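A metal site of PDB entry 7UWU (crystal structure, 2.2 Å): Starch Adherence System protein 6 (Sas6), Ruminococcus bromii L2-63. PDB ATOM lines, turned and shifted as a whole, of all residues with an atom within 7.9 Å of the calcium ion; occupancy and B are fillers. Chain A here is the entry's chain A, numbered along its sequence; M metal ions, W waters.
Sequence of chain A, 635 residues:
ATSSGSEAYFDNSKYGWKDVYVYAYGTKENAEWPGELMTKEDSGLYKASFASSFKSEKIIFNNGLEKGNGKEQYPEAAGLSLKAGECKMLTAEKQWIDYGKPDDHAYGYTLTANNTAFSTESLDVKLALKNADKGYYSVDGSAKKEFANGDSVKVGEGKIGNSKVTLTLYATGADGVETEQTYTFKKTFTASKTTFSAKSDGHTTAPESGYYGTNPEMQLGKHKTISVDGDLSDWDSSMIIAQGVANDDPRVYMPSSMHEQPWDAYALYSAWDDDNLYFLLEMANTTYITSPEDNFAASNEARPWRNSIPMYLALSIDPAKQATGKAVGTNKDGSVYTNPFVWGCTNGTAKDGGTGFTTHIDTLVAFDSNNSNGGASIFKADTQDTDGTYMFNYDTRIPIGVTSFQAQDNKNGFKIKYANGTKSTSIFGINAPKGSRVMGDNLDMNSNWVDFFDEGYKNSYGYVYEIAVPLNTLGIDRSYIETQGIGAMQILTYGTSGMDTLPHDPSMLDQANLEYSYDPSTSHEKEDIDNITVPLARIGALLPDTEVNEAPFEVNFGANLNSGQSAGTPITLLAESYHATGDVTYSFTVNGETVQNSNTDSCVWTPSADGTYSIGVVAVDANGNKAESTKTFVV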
ATOM      1  N   THR A 225       4.088   6.593 -19.901  1.00  0.00           N
ATOM      2  CA  THR A 225       4.542   7.088 -21.192  1.00  0.00           C
ATOM      3  C   THR A 225       4.144   6.077 -22.269  1.00  0.00           C
ATOM      4  O   THR A 225       4.401   4.883 -22.133  1.00  0.00           O
ATOM      5  CB  THR A 225       6.063   7.284 -21.207  1.00  0.00           C
ATOM      6  OG1 THR A 225       6.456   8.248 -20.197  1.00  0.00           O
ATOM      7  CG2 THR A 225       6.531   7.770 -22.596  1.00  0.00           C
ATOM      8  N   ILE A 226       3.489   6.569 -23.326  1.00  0.00           N
ATOM      9  CA  ILE A 226       3.031   5.721 -24.424  1.00  0.00           C
ATOM     10  C   ILE A 226       3.870   6.044 -25.645  1.00  0.00           C
ATOM     11  O   ILE A 226       4.205   7.209 -25.870  1.00  0.00           O
ATOM     12  CB  ILE A 226       1.513   5.922 -24.715  1.00  0.00           C
ATOM     13  CG1 ILE A 226       0.648   5.310 -23.599  1.00  0.00           C
ATOM     14  CG2 ILE A 226       1.121   5.375 -26.104  1.00  0.00           C
ATOM     15  CD1 ILE A 226       0.586   3.781 -23.569  1.00  0.00           C
ATOM     16  N   SER A 227       4.191   5.024 -26.423  1.00  0.00           N
ATOM     17  CA  SER A 227       4.934   5.209 -27.666  1.00  0.00           C
ATOM     18  C   SER A 227       3.943   5.224 -28.821  1.00  0.00           C
ATOM     19  O   SER A 227       3.363   4.185 -29.177  1.00  0.00           O
ATOM     20  CB  SER A 227       5.985   4.125 -27.852  1.00  0.00           C
ATOM     21  OG  SER A 227       6.741   4.375 -29.034  1.00  0.00           O
ATOM     22  N   VAL A 228       3.734   6.403 -29.413  1.00  0.00           N
ATOM     23  CA  VAL A 228       2.795   6.545 -30.511  1.00  0.00           C
ATOM     24  C   VAL A 228       3.434   5.999 -31.787  1.00  0.00           C
ATOM     25  O   VAL A 228       3.983   6.755 -32.604  1.00  0.00           O
ATOM     26  CB  VAL A 228       2.337   8.005 -30.700  1.00  0.00           C
ATOM     27  CG1 VAL A 228       1.467   8.107 -31.905  1.00  0.00           C
ATOM     28  CG2 VAL A 228       1.538   8.445 -29.472  1.00  0.00           C
ATOM     29  N   ASP A 229       3.389   4.678 -31.928  1.00  0.00           N
ATOM     30  CA  ASP A 229       3.764   3.931 -33.113  1.00  0.00           C
ATOM     31  C   ASP A 229       2.459   3.307 -33.616  1.00  0.00           C
ATOM     32  O   ASP A 229       1.379   3.860 -33.372  1.00  0.00           O
ATOM     33  CB  ASP A 229       4.837   2.923 -32.725  1.00  0.00           C
ATOM     34  CG  ASP A 229       4.485   2.164 -31.466  1.00  0.00           C
ATOM     35  OD1 ASP A 229       3.267   1.997 -31.244  1.00  0.00           O
ATOM     36  OD2 ASP A 229       5.387   1.706 -30.733  1.00  0.00           O
ATOM     37  N   GLY A 230       2.528   2.151 -34.242  1.00  0.00           N
ATOM     38  CA  GLY A 230       1.265   1.466 -34.398  1.00  0.00           C
ATOM     39  C   GLY A 230       1.150   0.247 -33.533  1.00  0.00           C
ATOM     40  O   GLY A 230       0.230  -0.557 -33.716  1.00  0.00           O
ATOM     41  N   ASP A 231       2.072   0.073 -32.595  1.00  0.00           N
ATOM     42  CA  ASP A 231       2.178  -1.143 -31.805  1.00  0.00           C
ATOM     43  C   ASP A 231       1.366  -0.983 -30.522  1.00  0.00           C
ATOM     44  O   ASP A 231       1.281   0.118 -29.967  1.00  0.00           O
ATOM     45  CB  ASP A 231       3.656  -1.406 -31.510  1.00  0.00           C
ATOM     46  CG  ASP A 231       3.856  -2.476 -30.505  1.00  0.00           C
ATOM     47  OD1 ASP A 231       3.814  -3.672 -30.893  1.00  0.00           O
ATOM     48  OD2 ASP A 231       4.016  -2.112 -29.330  1.00  0.00           O
ATOM     49  N   LEU A 232       0.757  -2.068 -30.077  1.00  0.00           N
ATOM     50  CA  LEU A 232      -0.175  -2.019 -28.955  1.00  0.00           C
ATOM     51  C   LEU A 232       0.367  -2.736 -27.710  1.00  0.00           C
ATOM     52  O   LEU A 232      -0.396  -2.977 -26.755  1.00  0.00           O
ATOM     53  CB  LEU A 232      -1.533  -2.582 -29.368  1.00  0.00           C
ATOM     54  CG  LEU A 232      -2.000  -2.258 -30.796  1.00  0.00           C
ATOM     55  CD1 LEU A 232      -3.096  -3.208 -31.268  1.00  0.00           C
ATOM     56  CD2 LEU A 232      -2.484  -0.827 -30.911  1.00  0.00           C
ATOM     57  N   SER A 233       1.672  -3.047 -27.689  1.00  0.00           N
ATOM     58  CA  SER A 233       2.242  -3.717 -26.532  1.00  0.00           C
ATOM     59  C   SER A 233       2.292  -2.809 -25.309  1.00  0.00           C
ATOM     60  O   SER A 233       2.449  -3.304 -24.187  1.00  0.00           O
ATOM     61  CB  SER A 233       3.652  -4.238 -26.853  1.00  0.00           C
ATOM     62  OG  SER A 233       4.526  -3.171 -27.197  1.00  0.00           O
ATOM     63  N   ASP A 234       2.159  -1.493 -25.491  1.00  0.00           N
ATOM     64  CA  ASP A 234       2.169  -0.559 -24.372  1.00  0.00           C
ATOM     65  C   ASP A 234       0.772  -0.306 -23.786  1.00  0.00           C
ATOM     66  O   ASP A 234       0.626   0.582 -22.945  1.00  0.00           O
ATOM     67  CB  ASP A 234       2.820   0.777 -24.788  1.00  0.00           C
ATOM     68  CG  ASP A 234       2.456   1.190 -26.196  1.00  0.00           C
ATOM     69  OD1 ASP A 234       1.753   0.395 -26.862  1.00  0.00           O
ATOM     70  OD2 ASP A 234       2.866   2.291 -26.636  1.00  0.00           O
ATOM     71  N   TRP A 235      -0.255  -1.064 -24.194  1.00  0.00           N
ATOM     72  CA  TRP A 235      -1.604  -0.913 -23.656  1.00  0.00           C
ATOM     73  C   TRP A 235      -2.113  -2.236 -23.092  1.00  0.00           C
ATOM     74  O   TRP A 235      -1.698  -3.312 -23.505  1.00  0.00           O
ATOM     75  CB  TRP A 235      -2.592  -0.447 -24.742  1.00  0.00           C
ATOM     76  CG  TRP A 235      -2.281   0.899 -25.377  1.00  0.00           C
ATOM     77  CD1 TRP A 235      -1.533   1.126 -26.476  1.00  0.00           C
ATOM     78  CD2 TRP A 235      -2.760   2.191 -24.941  1.00  0.00           C
ATOM     79  NE1 TRP A 235      -1.490   2.471 -26.755  1.00  0.00           N
ATOM     80  CE2 TRP A 235      -2.228   3.140 -25.826  1.00  0.00           C
ATOM     81  CE3 TRP A 235      -3.568   2.616 -23.880  1.00  0.00           C
ATOM     82  CZ2 TRP A 235      -2.478   4.506 -25.699  1.00  0.00           C
ATOM     83  CZ3 TRP A 235      -3.811   3.980 -23.746  1.00  0.00           C
ATOM     84  CH2 TRP A 235      -3.268   4.905 -24.649  1.00  0.00           C
ATOM     85  N   LEU A 280      -5.717   5.218 -27.241  1.00  0.00           N
ATOM     86  CA  LEU A 280      -5.849   4.137 -28.194  1.00  0.00           C
ATOM     87  C   LEU A 280      -7.327   3.998 -28.520  1.00  0.00           C
ATOM     88  O   LEU A 280      -8.174   4.051 -27.612  1.00  0.00           O
ATOM     89  CB  LEU A 280      -5.291   2.833 -27.606  1.00  0.00           C
ATOM     90  CG  LEU A 280      -5.592   1.559 -28.392  1.00  0.00           C
ATOM     91  CD1 LEU A 280      -4.896   1.675 -29.718  1.00  0.00           C
ATOM     92  CD2 LEU A 280      -5.125   0.307 -27.635  1.00  0.00           C
ATOM     93  N   GLU A 466      -3.584   5.309 -32.557  1.00  0.00           N
ATOM     94  CA  GLU A 466      -2.796   5.690 -31.395  1.00  0.00           C
ATOM     95  C   GLU A 466      -2.483   7.173 -31.500  1.00  0.00           C
ATOM     96  O   GLU A 466      -1.953   7.618 -32.529  1.00  0.00           O
ATOM     97  CB  GLU A 466      -1.507   4.862 -31.330  1.00  0.00           C
ATOM     98  CG  GLU A 466      -1.141   4.467 -29.935  1.00  0.00           C
ATOM     99  CD  GLU A 466      -0.039   3.409 -29.846  1.00  0.00           C
ATOM    100  OE1 GLU A 466       0.582   3.098 -30.880  1.00  0.00           O
ATOM    101  OE2 GLU A 466       0.188   2.881 -28.722  1.00  0.00           O
HETATM  102 CA    CA M   1       2.356   1.964 -28.929  1.00  0.00          CA
HETATM  103  O   HOH W   1       4.575   0.354 -28.229  1.00  0.00           O
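OD2 of Asp 231 sits at hydrogen-bond distance from OG of Ser 233, at 2.4 Å. The side-chain carboxylate (OE2) of Glu 466 lies close to the indole nitrogen (NE1) of Trp 235, 2.6 Å away.
Of the 13 residues printed, 5 come within 4 Å of the calcium ion. The nearest printed residue that does not touch the calcium ion is Trp 235 (4.4 Å).
The calcium ion is bound by the side-chain carboxylate (OE2) of Glu 466 (2.4 Å), the side-chain carboxylate (OD2) of Asp 234 (2.4 Å), the backbone carbonyl oxygen (O) of Asp 231 (2.4 Å), the backbone carbonyl oxygen (O) of Ser 227 (2.5 Å), the side-chain carboxylate (OD1) of Asp 229 (2.5 Å), the side-chain carboxylate (OD1) of Asp 234 (2.7 Å), water W1 (2.8 Å) and the side-chain carboxylate (OE1) of Glu 466 (2.9 Å). The calcium ion has eight donor atoms within binding distance.
Water W1 bridges the side-chain carboxylate (OD2) of Asp 231 and the side-chain carboxylate (OD2) of Asp 229.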
